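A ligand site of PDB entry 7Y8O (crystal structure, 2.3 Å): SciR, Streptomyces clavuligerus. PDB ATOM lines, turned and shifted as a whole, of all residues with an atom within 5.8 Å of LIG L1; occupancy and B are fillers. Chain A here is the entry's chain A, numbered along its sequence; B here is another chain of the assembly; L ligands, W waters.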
ATOM      1  N   GLY A  11      11.154  29.780  15.185  1.00  0.00           N
ATOM      2  CA  GLY A  11      11.940  30.114  14.010  1.00  0.00           C
ATOM      3  C   GLY A  11      11.108  30.014  12.752  1.00  0.00           C
ATOM      4  O   GLY A  11      10.871  28.910  12.241  1.00  0.00           O
ATOM      5  N   LEU A  12      10.662  31.154  12.231  1.00  0.00           N
ATOM      6  CA  LEU A  12       9.726  31.195  11.123  1.00  0.00           C
ATOM      7  C   LEU A  12      10.328  31.895   9.907  1.00  0.00           C
ATOM      8  O   LEU A  12       9.702  32.736   9.269  1.00  0.00           O
ATOM      9  CB  LEU A  12       8.425  31.874  11.543  1.00  0.00           C
ATOM     10  CG  LEU A  12       7.610  31.032  12.523  1.00  0.00           C
ATOM     11  CD1 LEU A  12       6.294  31.700  12.859  1.00  0.00           C
ATOM     12  CD2 LEU A  12       7.384  29.639  11.975  1.00  0.00           C
ATOM     13  N   GLY A  13      11.568  31.532   9.565  1.00  0.00           N
ATOM     14  CA  GLY A  13      12.141  31.933   8.304  1.00  0.00           C
ATOM     15  C   GLY A  13      11.578  31.087   7.182  1.00  0.00           C
ATOM     16  O   GLY A  13      10.572  30.394   7.357  1.00  0.00           O
ATOM     17  N   PRO A  14      12.209  31.140   6.000  1.00  0.00           N
ATOM     18  CA  PRO A  14      11.702  30.348   4.867  1.00  0.00           C
ATOM     19  C   PRO A  14      11.435  28.890   5.194  1.00  0.00           C
ATOM     20  O   PRO A  14      10.390  28.353   4.782  1.00  0.00           O
ATOM     21  CB  PRO A  14      12.806  30.491   3.816  1.00  0.00           C
ATOM     22  CG  PRO A  14      13.530  31.734   4.160  1.00  0.00           C
ATOM     23  CD  PRO A  14      13.240  32.108   5.591  1.00  0.00           C
ATOM     24  N   MET A  15      12.331  28.226   5.913  1.00  0.00           N
ATOM     25  CA  MET A  15      12.103  26.829   6.287  1.00  0.00           C
ATOM     26  C   MET A  15      11.000  26.718   7.336  1.00  0.00           C
ATOM     27  O   MET A  15      10.097  25.894   7.205  1.00  0.00           O
ATOM     28  CB  MET A  15      13.390  26.199   6.802  1.00  0.00           C
ATOM     29  CG  MET A  15      14.453  25.963   5.741  1.00  0.00           C
ATOM     30  SD  MET A  15      13.849  24.999   4.341  1.00  0.00           S
ATOM     31  CE  MET A  15      14.071  23.345   4.975  1.00  0.00           C
ATOM     32  N   GLY A  16      11.074  27.536   8.393  1.00  0.00           N
ATOM     33  CA  GLY A  16      10.072  27.451   9.454  1.00  0.00           C
ATOM     34  C   GLY A  16       8.658  27.710   8.965  1.00  0.00           C
ATOM     35  O   GLY A  16       7.719  27.044   9.404  1.00  0.00           O
ATOM     36  N   ASN A  34       8.078  33.452  17.106  1.00  0.00           N
ATOM     37  CA  ASN A  34       9.141  33.997  16.280  1.00  0.00           C
ATOM     38  C   ASN A  34       9.581  35.341  16.847  1.00  0.00           C
ATOM     39  O   ASN A  34       8.772  36.060  17.444  1.00  0.00           O
ATOM     40  CB  ASN A  34       8.690  34.151  14.828  1.00  0.00           C
ATOM     41  CG  ASN A  34       9.849  34.292  13.859  1.00  0.00           C
ATOM     42  OD1 ASN A  34      10.727  33.435  13.796  1.00  0.00           O
ATOM     43  ND2 ASN A  34       9.856  35.390  13.104  1.00  0.00           N
ATOM     44  N   ARG A  35      10.861  35.670  16.666  1.00  0.00           N
ATOM     45  CA  ARG A  35      11.362  36.963  17.110  1.00  0.00           C
ATOM     46  C   ARG A  35      10.627  38.097  16.396  1.00  0.00           C
ATOM     47  O   ARG A  35      10.149  39.042  17.033  1.00  0.00           O
ATOM     48  CB  ARG A  35      12.870  37.054  16.881  1.00  0.00           C
ATOM     49  CG  ARG A  35      13.413  38.478  16.933  1.00  0.00           C
ATOM     50  CD  ARG A  35      14.912  38.521  16.681  1.00  0.00           C
ATOM     51  NE  ARG A  35      15.251  38.152  15.318  1.00  0.00           N
ATOM     52  CZ  ARG A  35      16.480  38.173  14.816  1.00  0.00           C
ATOM     53  NH1 ARG A  35      17.514  38.552  15.547  1.00  0.00           N
ATOM     54  NH2 ARG A  35      16.673  37.798  13.549  1.00  0.00           N
ATOM     55  N   THR A  36      10.532  38.017  15.067  1.00  0.00           N
ATOM     56  CA  THR A  36       9.704  38.928  14.293  1.00  0.00           C
ATOM     57  C   THR A  36       8.298  38.327  14.269  1.00  0.00           C
ATOM     58  O   THR A  36       7.994  37.451  13.462  1.00  0.00           O
ATOM     59  CB  THR A  36      10.261  39.128  12.886  1.00  0.00           C
ATOM     60  OG1 THR A  36      11.652  39.453  12.970  1.00  0.00           O
ATOM     61  CG2 THR A  36       9.525  40.253  12.183  1.00  0.00           C
ATOM     62  N   ARG A  39       5.814  37.390  11.219  1.00  0.00           N
ATOM     63  CA  ARG A  39       5.964  36.243  10.342  1.00  0.00           C
ATOM     64  C   ARG A  39       5.087  35.052  10.754  1.00  0.00           C
ATOM     65  O   ARG A  39       5.031  34.070  10.008  1.00  0.00           O
ATOM     66  CB  ARG A  39       7.428  35.815  10.290  1.00  0.00           C
ATOM     67  CG  ARG A  39       8.332  36.902   9.743  1.00  0.00           C
ATOM     68  CD  ARG A  39       9.783  36.457   9.732  1.00  0.00           C
ATOM     69  NE  ARG A  39      10.226  36.118   8.393  1.00  0.00           N
ATOM     70  CZ  ARG A  39      11.461  35.729   8.084  1.00  0.00           C
ATOM     71  NH1 ARG A  39      12.402  35.642   9.010  1.00  0.00           N
ATOM     72  NH2 ARG A  39      11.753  35.422   6.826  1.00  0.00           N
ATOM     73  N   SER A  67      14.088  26.113  13.929  1.00  0.00           N
ATOM     74  CA  SER A  67      14.603  26.366  12.576  1.00  0.00           C
ATOM     75  C   SER A  67      15.242  27.748  12.623  1.00  0.00           C
ATOM     76  O   SER A  67      14.599  28.751  12.286  1.00  0.00           O
ATOM     77  CB  SER A  67      13.497  26.283  11.529  1.00  0.00           C
ATOM     78  OG  SER A  67      14.033  26.318  10.215  1.00  0.00           O
ATOM     79  N   LEU A  68      16.502  27.805  13.044  1.00  0.00           N
ATOM     80  CA  LEU A  68      17.214  29.065  13.225  1.00  0.00           C
ATOM     81  C   LEU A  68      18.465  29.071  12.357  1.00  0.00           C
ATOM     82  O   LEU A  68      18.837  28.055  11.753  1.00  0.00           O
ATOM     83  CB  LEU A  68      17.576  29.273  14.706  1.00  0.00           C
ATOM     84  CG  LEU A  68      16.372  29.244  15.665  1.00  0.00           C
ATOM     85  CD1 LEU A  68      16.827  29.090  17.109  1.00  0.00           C
ATOM     86  CD2 LEU A  68      15.497  30.484  15.487  1.00  0.00           C
ATOM     87  N   THR A  69      19.113  30.234  12.293  1.00  0.00           N
ATOM     88  CA  THR A  69      20.266  30.381  11.410  1.00  0.00           C
ATOM     89  C   THR A  69      21.423  29.479  11.830  1.00  0.00           C
ATOM     90  O   THR A  69      22.028  28.799  10.997  1.00  0.00           O
ATOM     91  CB  THR A  69      20.707  31.841  11.355  1.00  0.00           C
ATOM     92  OG1 THR A  69      19.627  32.656  10.880  1.00  0.00           O
ATOM     93  CG2 THR A  69      21.901  32.022  10.434  1.00  0.00           C
ATOM     94  N   ASP A  70      21.723  29.445  13.122  1.00  0.00           N
ATOM     95  CA  ASP A  70      22.767  28.577  13.640  1.00  0.00           C
ATOM     96  C   ASP A  70      22.443  28.234  15.093  1.00  0.00           C
ATOM     97  O   ASP A  70      21.366  28.566  15.605  1.00  0.00           O
ATOM     98  CB  ASP A  70      24.151  29.228  13.471  1.00  0.00           C
ATOM     99  CG  ASP A  70      24.243  30.590  14.135  1.00  0.00           C
ATOM    100  OD1 ASP A  70      23.295  30.984  14.849  1.00  0.00           O
ATOM    101  OD2 ASP A  70      25.273  31.275  13.939  1.00  0.00           O
ATOM    102  N   ASP A  72      24.061  29.319  17.792  1.00  0.00           N
ATOM    103  CA  ASP A  72      24.153  30.475  18.685  1.00  0.00           C
ATOM    104  C   ASP A  72      22.792  31.125  18.878  1.00  0.00           C
ATOM    105  O   ASP A  72      22.504  31.651  19.964  1.00  0.00           O
ATOM    106  CB  ASP A  72      25.152  31.490  18.134  1.00  0.00           C
ATOM    107  CG  ASP A  72      26.586  31.129  18.452  1.00  0.00           C
ATOM    108  OD1 ASP A  72      26.814  30.373  19.425  1.00  0.00           O
ATOM    109  OD2 ASP A  72      27.496  31.584  17.727  1.00  0.00           O
ATOM    110  N   ALA A  73      21.932  31.098  17.856  1.00  0.00           N
ATOM    111  CA  ALA A  73      20.575  31.601  17.997  1.00  0.00           C
ATOM    112  C   ALA A  73      19.758  30.769  18.976  1.00  0.00           C
ATOM    113  O   ALA A  73      18.792  31.290  19.559  1.00  0.00           O
ATOM    114  CB  ALA A  73      19.890  31.652  16.630  1.00  0.00           C
ATOM    115  N   ALA A  76      20.594  32.164  22.286  1.00  0.00           N
ATOM    116  CA  ALA A  76      20.027  33.504  22.392  1.00  0.00           C
ATOM    117  C   ALA A  76      18.537  33.450  22.682  1.00  0.00           C
ATOM    118  O   ALA A  76      18.020  34.255  23.457  1.00  0.00           O
ATOM    119  CB  ALA A  76      20.306  34.291  21.114  1.00  0.00           C
ATOM    120  N   LEU A  77      17.825  32.493  22.075  1.00  0.00           N
ATOM    121  CA  LEU A  77      16.384  32.416  22.247  1.00  0.00           C
ATOM    122  C   LEU A  77      15.994  31.627  23.494  1.00  0.00           C
ATOM    123  O   LEU A  77      15.120  32.048  24.252  1.00  0.00           O
ATOM    124  CB  LEU A  77      15.739  31.800  21.010  1.00  0.00           C
ATOM    125  CG  LEU A  77      15.390  32.765  19.872  1.00  0.00           C
ATOM    126  CD1 LEU A  77      14.500  32.079  18.846  1.00  0.00           C
ATOM    127  CD2 LEU A  77      14.744  34.027  20.413  1.00  0.00           C
ATOM    128  N   LEU A  93      16.763  21.891  13.986  1.00  0.00           N
ATOM    129  CA  LEU A  93      16.961  21.734  12.548  1.00  0.00           C
ATOM    130  C   LEU A  93      17.792  22.867  11.951  1.00  0.00           C
ATOM    131  O   LEU A  93      17.595  23.236  10.792  1.00  0.00           O
ATOM    132  CB  LEU A  93      15.620  21.630  11.835  1.00  0.00           C
ATOM    133  CG  LEU A  93      14.654  20.568  12.373  1.00  0.00           C
ATOM    134  CD1 LEU A  93      13.355  20.561  11.572  1.00  0.00           C
ATOM    135  CD2 LEU A  93      15.313  19.206  12.358  1.00  0.00           C
ATOM    136  N   SER A  94      18.723  23.419  12.730  1.00  0.00           N
ATOM    137  CA  SER A  94      19.582  24.505  12.284  1.00  0.00           C
ATOM    138  C   SER A  94      20.940  23.961  11.891  1.00  0.00           C
ATOM    139  O   SER A  94      21.458  23.030  12.529  1.00  0.00           O
ATOM    140  CB  SER A  94      19.746  25.569  13.364  1.00  0.00           C
ATOM    141  OG  SER A  94      18.521  25.824  14.034  1.00  0.00           O
ATOM    142  N   SER A  95      21.521  24.532  10.843  1.00  0.00           N
ATOM    143  CA  SER A  95      22.863  24.146  10.419  1.00  0.00           C
ATOM    144  C   SER A  95      23.899  24.651  11.408  1.00  0.00           C
ATOM    145  O   SER A  95      23.774  25.740  11.968  1.00  0.00           O
ATOM    146  CB  SER A  95      23.154  24.704   9.032  1.00  0.00           C
ATOM    147  OG  SER A  95      24.465  24.351   8.601  1.00  0.00           O
ATOM    148  N   VAL A 120      18.040  19.215   7.359  1.00  0.00           N
ATOM    149  CA  VAL A 120      17.042  19.085   6.312  1.00  0.00           C
ATOM    150  C   VAL A 120      17.690  19.382   4.963  1.00  0.00           C
ATOM    151  O   VAL A 120      18.284  20.456   4.780  1.00  0.00           O
ATOM    152  CB  VAL A 120      15.854  20.030   6.564  1.00  0.00           C
ATOM    153  CG1 VAL A 120      14.715  19.717   5.609  1.00  0.00           C
ATOM    154  CG2 VAL A 120      15.379  19.901   8.015  1.00  0.00           C
ATOM    155  N   THR A 121      17.577  18.443   4.031  1.00  0.00           N
ATOM    156  CA  THR A 121      18.265  18.541   2.740  1.00  0.00           C
ATOM    157  C   THR A 121      17.328  18.933   1.601  1.00  0.00           C
ATOM    158  O   THR A 121      17.564  18.558   0.444  1.00  0.00           O
ATOM    159  CB  THR A 121      18.954  17.215   2.402  1.00  0.00           C
ATOM    160  OG1 THR A 121      17.976  16.196   2.174  1.00  0.00           O
ATOM    161  CG2 THR A 121      19.867  16.787   3.544  1.00  0.00           C
ATOM    162  N   CYS A 122      16.296  19.713   1.886  1.00  0.00           N
ATOM    163  CA  CYS A 122      15.363  20.171   0.866  1.00  0.00           C
ATOM    164  C   CYS A 122      15.036  21.635   1.087  1.00  0.00           C
ATOM    165  O   CYS A 122      15.160  22.153   2.205  1.00  0.00           O
ATOM    166  CB  CYS A 122      14.066  19.337   0.903  1.00  0.00           C
ATOM    167  SG  CYS A 122      13.086  19.583   2.381  1.00  0.00           S
ATOM    168  N   PRO A 123      14.624  22.339   0.030  1.00  0.00           N
ATOM    169  CA  PRO A 123      14.225  23.740   0.178  1.00  0.00           C
ATOM    170  C   PRO A 123      12.857  23.852   0.835  1.00  0.00           C
ATOM    171  O   PRO A 123      12.199  22.826   1.073  1.00  0.00           O
ATOM    172  CB  PRO A 123      14.177  24.233  -1.277  1.00  0.00           C
ATOM    173  CG  PRO A 123      13.825  23.015  -2.056  1.00  0.00           C
ATOM    174  CD  PRO A 123      14.568  21.897  -1.373  1.00  0.00           C
ATOM    175  N   PRO A 124      12.410  25.070   1.175  1.00  0.00           N
ATOM    176  CA  PRO A 124      11.078  25.216   1.803  1.00  0.00           C
ATOM    177  C   PRO A 124       9.948  24.555   1.038  1.00  0.00           C
ATOM    178  O   PRO A 124       9.086  23.910   1.646  1.00  0.00           O
ATOM    179  CB  PRO A 124      10.906  26.735   1.895  1.00  0.00           C
ATOM    180  CG  PRO A 124      12.294  27.252   1.995  1.00  0.00           C
ATOM    181  CD  PRO A 124      13.104  26.366   1.089  1.00  0.00           C
ATOM    182  N   TYR A 170      25.026  16.721   6.904  1.00  0.00           N
ATOM    183  CA  TYR A 170      24.498  17.904   6.229  1.00  0.00           C
ATOM    184  C   TYR A 170      25.606  18.699   5.549  1.00  0.00           C
ATOM    185  O   TYR A 170      25.434  19.186   4.425  1.00  0.00           O
ATOM    186  CB  TYR A 170      23.739  18.789   7.226  1.00  0.00           C
ATOM    187  CG  TYR A 170      23.067  19.984   6.581  1.00  0.00           C
ATOM    188  CD1 TYR A 170      21.869  19.849   5.906  1.00  0.00           C
ATOM    189  CD2 TYR A 170      23.648  21.251   6.643  1.00  0.00           C
ATOM    190  CE1 TYR A 170      21.258  20.933   5.311  1.00  0.00           C
ATOM    191  CE2 TYR A 170      23.030  22.345   6.055  1.00  0.00           C
ATOM    192  CZ  TYR A 170      21.838  22.181   5.385  1.00  0.00           C
ATOM    193  OH  TYR A 170      21.229  23.255   4.792  1.00  0.00           O
ATOM    194  N   ALA B 232      13.087  32.474  -0.386  1.00  0.00           N
ATOM    195  CA  ALA B 232      13.579  31.114  -0.236  1.00  0.00           C
ATOM    196  C   ALA B 232      14.888  31.033   0.532  1.00  0.00           C
ATOM    197  O   ALA B 232      15.169  29.982   1.122  1.00  0.00           O
ATOM    198  CB  ALA B 232      13.769  30.454  -1.614  1.00  0.00           C
ATOM    199  N   ASP B 233      15.678  32.097   0.533  1.00  0.00           N
ATOM    200  CA  ASP B 233      16.968  32.079   1.221  1.00  0.00           C
ATOM    201  C   ASP B 233      17.451  33.513   1.400  1.00  0.00           C
ATOM    202  O   ASP B 233      17.221  34.364   0.540  1.00  0.00           O
ATOM    203  CB  ASP B 233      18.005  31.273   0.440  1.00  0.00           C
ATOM    204  CG  ASP B 233      18.479  31.997  -0.817  1.00  0.00           C
ATOM    205  OD1 ASP B 233      17.743  31.992  -1.826  1.00  0.00           O
ATOM    206  OD2 ASP B 233      19.586  32.580  -0.779  1.00  0.00           O
ATOM    207  N   ARG B 234      18.105  33.773   2.526  1.00  0.00           N
ATOM    208  CA  ARG B 234      18.820  35.009   2.744  1.00  0.00           C
ATOM    209  C   ARG B 234      20.320  34.761   2.605  1.00  0.00           C
ATOM    210  O   ARG B 234      20.824  33.720   3.023  1.00  0.00           O
ATOM    211  CB  ARG B 234      18.522  35.603   4.130  1.00  0.00           C
ATOM    212  CG  ARG B 234      17.110  36.149   4.286  1.00  0.00           C
ATOM    213  CD  ARG B 234      16.789  36.387   5.758  1.00  0.00           C
ATOM    214  NE  ARG B 234      17.740  37.291   6.384  1.00  0.00           N
ATOM    215  CZ  ARG B 234      18.631  36.927   7.298  1.00  0.00           C
ATOM    216  NH1 ARG B 234      18.722  35.667   7.703  1.00  0.00           N
ATOM    217  NH2 ARG B 234      19.447  37.839   7.814  1.00  0.00           N
ATOM    218  N   MET B 237      22.088  33.952   5.769  1.00  0.00           N
ATOM    219  CA  MET B 237      21.952  32.565   6.186  1.00  0.00           C
ATOM    220  C   MET B 237      22.941  31.673   5.445  1.00  0.00           C
ATOM    221  O   MET B 237      23.507  30.743   6.028  1.00  0.00           O
ATOM    222  CB  MET B 237      20.521  32.088   5.973  1.00  0.00           C
ATOM    223  CG  MET B 237      20.295  30.601   6.256  1.00  0.00           C
ATOM    224  SD  MET B 237      20.561  29.508   4.828  1.00  0.00           S
ATOM    225  CE  MET B 237      19.617  30.357   3.570  1.00  0.00           C
ATOM    226  N   SER B 241      26.050  29.175   6.667  1.00  0.00           N
ATOM    227  CA  SER B 241      26.112  27.802   6.178  1.00  0.00           C
ATOM    228  C   SER B 241      27.503  27.476   5.627  1.00  0.00           C
ATOM    229  O   SER B 241      28.073  26.428   5.932  1.00  0.00           O
ATOM    230  CB  SER B 241      25.037  27.587   5.112  1.00  0.00           C
ATOM    231  OG  SER B 241      25.179  26.331   4.484  1.00  0.00           O
ATOM    232  N   HIS B 244      29.911  27.238   8.348  1.00  0.00           N
ATOM    233  CA  HIS B 244      29.853  25.944   9.029  1.00  0.00           C
ATOM    234  C   HIS B 244      30.664  24.894   8.294  1.00  0.00           C
ATOM    235  O   HIS B 244      31.355  24.086   8.915  1.00  0.00           O
ATOM    236  CB  HIS B 244      28.394  25.489   9.168  1.00  0.00           C
ATOM    237  CG  HIS B 244      27.525  26.451   9.894  1.00  0.00           C
ATOM    238  ND1 HIS B 244      26.169  26.556   9.668  1.00  0.00           N
ATOM    239  CD2 HIS B 244      27.818  27.374  10.847  1.00  0.00           C
ATOM    240  CE1 HIS B 244      25.663  27.491  10.449  1.00  0.00           C
ATOM    241  NE2 HIS B 244      26.643  28.003  11.176  1.00  0.00           N
HETATM  242  P1  LIG L   1      17.007  32.133   8.332  1.00  0.00           P
HETATM  243  O1  LIG L   1      17.039  33.286   7.405  1.00  0.00           O
HETATM  244  O2  LIG L   1      18.281  31.469   8.698  1.00  0.00           O
HETATM  245  O3  LIG L   1      16.242  32.549   9.665  1.00  0.00           O
HETATM  246  C1  LIG L   1      15.601  31.504  10.412  1.00  0.00           C
HETATM  247  C2  LIG L   1      15.043  32.064  11.688  1.00  0.00           C
HETATM  248  O4  LIG L   1      16.132  32.346  12.599  1.00  0.00           O
HETATM  249  C3  LIG L   1      14.238  33.377  11.582  1.00  0.00           C
HETATM  250  O5  LIG L   1      12.904  33.134  11.996  1.00  0.00           O
HETATM  251  C4  LIG L   1      15.002  34.369  12.455  1.00  0.00           C
HETATM  252  O6  LIG L   1      14.164  35.197  13.263  1.00  0.00           O
HETATM  253  C5  LIG L   1      15.751  33.440  13.393  1.00  0.00           C
HETATM  254  N1  LIG L   1      16.936  33.991  14.016  1.00  0.00           N
HETATM  255  C6  LIG L   1      18.190  34.095  13.474  1.00  0.00           C
HETATM  256  N2  LIG L   1      19.066  34.621  14.295  1.00  0.00           N
HETATM  257  C7  LIG L   1      18.345  34.885  15.440  1.00  0.00           C
HETATM  258  C8  LIG L   1      18.712  35.434  16.683  1.00  0.00           C
HETATM  259  N3  LIG L   1      19.941  35.847  16.983  1.00  0.00           N
HETATM  260  N4  LIG L   1      17.755  35.547  17.627  1.00  0.00           N
HETATM  261  C9  LIG L   1      16.517  35.130  17.323  1.00  0.00           C
HETATM  262  N5  LIG L   1      16.056  34.593  16.202  1.00  0.00           N
HETATM  263  C10 LIG L   1      17.032  34.491  15.288  1.00  0.00           C
HETATM  264  O7  LIG L   1      15.995  31.044   7.748  1.00  0.00           O
HETATM  265  P2  LIG L   1      16.031  29.705   6.887  1.00  0.00           P
HETATM  266  O8  LIG L   1      14.708  29.074   7.083  1.00  0.00           O
HETATM  267  O9  LIG L   1      16.473  30.007   5.505  1.00  0.00           O
HETATM  268  O10 LIG L   1      17.161  28.847   7.612  1.00  0.00           O
HETATM  269  C11 LIG L   1      16.842  28.023   8.751  1.00  0.00           C
HETATM  270  C12 LIG L   1      17.922  27.000   8.977  1.00  0.00           C
HETATM  271  O11 LIG L   1      17.718  25.887   8.071  1.00  0.00           O
HETATM  272  C13 LIG L   1      19.369  27.467   8.754  1.00  0.00           C
HETATM  273  O12 LIG L   1      20.235  26.911   9.738  1.00  0.00           O
HETATM  274  C14 LIG L   1      19.690  26.932   7.373  1.00  0.00           C
HETATM  275  O13 LIG L   1      21.063  26.676   7.141  1.00  0.00           O
HETATM  276  C15 LIG L   1      18.893  25.642   7.353  1.00  0.00           C
HETATM  277  N6  LIG L   1      18.482  25.306   5.972  1.00  0.00           N
HETATM  278  C16 LIG L   1      18.154  26.271   5.067  1.00  0.00           C
HETATM  279  C17 LIG L   1      17.357  25.969   4.009  1.00  0.00           C
HETATM  280  C18 LIG L   1      16.799  26.994   3.110  1.00  0.00           C
HETATM  281  O14 LIG L   1      16.419  26.665   1.987  1.00  0.00           O
HETATM  282  N7  LIG L   1      16.688  28.245   3.520  1.00  0.00           N
HETATM  283  C19 LIG L   1      17.048  24.567   3.777  1.00  0.00           C
HETATM  284  C20 LIG L   1      17.627  23.592   4.693  1.00  0.00           C
HETATM  285  C21 LIG L   1      18.422  23.996   5.630  1.00  0.00           C
HETATM  286  P3  LIG L   1      13.456  36.454  12.551  1.00  0.00           P
HETATM  287  O15 LIG L   1      14.413  37.137  11.652  1.00  0.00           O
HETATM  288  O16 LIG L   1      13.078  37.314  13.689  1.00  0.00           O
HETATM  289  O17 LIG L   1      12.251  35.961  11.825  1.00  0.00           O
HETATM  290  C1  LG2 L   2      19.652  22.586  -0.792  1.00  0.00           C
HETATM  291  C2  LG2 L   2      20.011  21.362  -0.017  1.00  0.00           C
HETATM  292  C3  LG2 L   2      18.920  23.503   0.171  1.00  0.00           C
HETATM  293  C4  LG2 L   2      19.716  21.718   1.436  1.00  0.00           C
HETATM  294  C5  LG2 L   2      19.159  24.991   0.239  1.00  0.00           C
HETATM  295  C6  LG2 L   2      18.621  25.822  -0.712  1.00  0.00           C
HETATM  296  C7  LG2 L   2      19.916  25.520   1.270  1.00  0.00           C
HETATM  297  C8  LG2 L   2      20.135  26.875   1.328  1.00  0.00           C
HETATM  298  C9  LG2 L   2      18.853  27.180  -0.658  1.00  0.00           C
HETATM  299  C10 LG2 L   2      19.612  27.718   0.362  1.00  0.00           C
HETATM  300  F1  LG2 L   2      20.878  27.393   2.320  1.00  0.00           F
HETATM  301  N1  LG2 L   2      18.615  22.644   1.331  1.00  0.00           N
HETATM  302  O   HOH W   1      17.081  32.446   4.737  1.00  0.00           O
HETATM  303  O   HOH W   2      17.451  36.481  20.195  1.00  0.00           O
HETATM  304  O   HOH W   3      18.570  21.919   8.166  1.00  0.00           O
HETATM  305  O   HOH W   4      15.564  24.328   8.991  1.00  0.00           O
HETATM  306  O   HOH W   5      16.101  36.886   9.703  1.00  0.00           O
HETATM  307  O   HOH W   6      22.656  28.684   8.094  1.00  0.00           O
HETATM  308  O   HOH W   7      12.784  33.911  15.645  1.00  0.00           O
HETATM  309  O   HOH W   8      13.195  29.105   9.391  1.00  0.00           O
HETATM  310  O   HOH W   9      22.149  25.655   4.811  1.00  0.00           O
HETATM  311  O   HOH W  10      21.956  35.217  13.375  1.00  0.00           O
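The backbone NH of Leu 12 lies within hydrogen-bond range of an oxygen (O5) of LIG L1 (3.0 Å).
The guanidinium group (NE) of Arg 35 is in salt-bridge range of an oxygen (O16) of LIG L1 (2.8 Å).
O of Thr 69 lies within hydrogen-bond range of O12 of LIG L1, at 2.9 Å.
O2 of LIG L1 lies within hydrogen-bond range of OG1 of Thr 69, 2.8 Å away.
An oxygen (O5) of LIG L1 is in hydrogen-bond range of the backbone NH (N) of Gly 13 (3.2 Å).
The guanidinium group (NH1) of Arg 39 is in salt-bridge range of an oxygen (O17) of LIG L1 (2.8 Å).
The backbone carbonyl oxygen (O) of Leu 68 is in hydrogen-bond range of an oxygen (O12) of LIG L1 (2.7 Å).
The backbone NH (N) of Thr 36 is in hydrogen-bond range of an oxygen (O16) of LIG L1, 3.0 Å away.
O13 of LIG L1 sits at hydrogen-bond distance from SD of Met 237 of chain B.
O16 of LIG L1 is in hydrogen-bond range of OG1 of Thr 36, at 2.7 Å.
The backbone NH of Ser 95 lies within hydrogen-bond range of an oxygen (O12) of LIG L1 (2.9 Å).
The guanidinium group (NH1) of Arg 234 of chain B is in salt-bridge range of an oxygen (O1) of LIG L1 (2.9 Å).
ND2 of Asn 34 sits at hydrogen-bond distance from O17 of LIG L1 (2.8 Å).
The backbone NH of Met 15 sits at hydrogen-bond distance from an oxygen (O8) of LIG L1 (2.8 Å).
O of Ala 232 of chain B sits at hydrogen-bond distance from N7 of LIG L1 (3.3 Å).
The side-chain amide oxygen (OD1) of Asn 34 lies within hydrogen-bond range of the backbone NH (N) of Leu 12.
The backbone NH (N) of Leu 68 sits at hydrogen-bond distance from the side-chain hydroxyl (OG) of Ser 94, at 3.0 Å.
ND1 of His 244 of chain B is in hydrogen-bond range of OG of Ser 95, 3.0 Å away.
The side-chain amide nitrogen (ND2) of Asn 34 lies within hydrogen-bond range of the backbone carbonyl oxygen (O) of Thr 36 (2.8 Å).
OD1 of Asp 70 lies within hydrogen-bond range of N of Ala 73.
Water W1 bridges O9 of LIG L1 and N of Arg 234 of chain B.
Water W6 lies within hydrogen-bond range of O13 of LIG L1 (2.7 Å), O of Thr 69 (3.0 Å) and O of Met 237 of chain B (3.0 Å).
Water W8 lies within hydrogen-bond range of O8 of LIG L1, N of Gly 16, N of Gly 13 and OG of Ser 67.
Water W4 lies within hydrogen-bond range of OG of Ser 67 (2.8 Å), O11 of LIG L1 (2.8 Å) and O of Leu 93 (2.9 Å).
Water W7 lies within hydrogen-bond range of the backbone NH (N) of Arg 35 (2.8 Å), the side-chain amide oxygen (OD1) of Asn 34 (2.8 Å) and an oxygen (O6) of LIG L1 (3.0 Å).
Water W3 lies within hydrogen-bond range of N of Val 120 (2.9 Å) and O of Leu 93 (3.1 Å).
The backbone nitrogen of Pro 14 lies close to an oxygen (O8) of LIG L1, at 3.4 Å.
Gly 11 touches LIG L1 (C to O5, 3.7 Å).
Ser 67 touches LIG L1 (O to C2, 3.4 Å).
Ala 73 touches LIG L1.
Leu 77 touches LIG L1 (CG to C9, 3.7 Å).
Leu 93 touches LIG L1 (O to O11, 3.8 Å).
Ser 94 touches LIG L1.
O of Val 120 touches C20 of LIG L1, 3.2 Å away.
Cys 122 touches LIG L1 (O to C19, 3.4 Å).
Pro 124 touches LIG L1.
OH of Tyr 170 touches C21 of LIG L1 (3.0 Å).
The nearest printed residue that does not touch LIG L1 is Pro 123 (4.1 Å).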
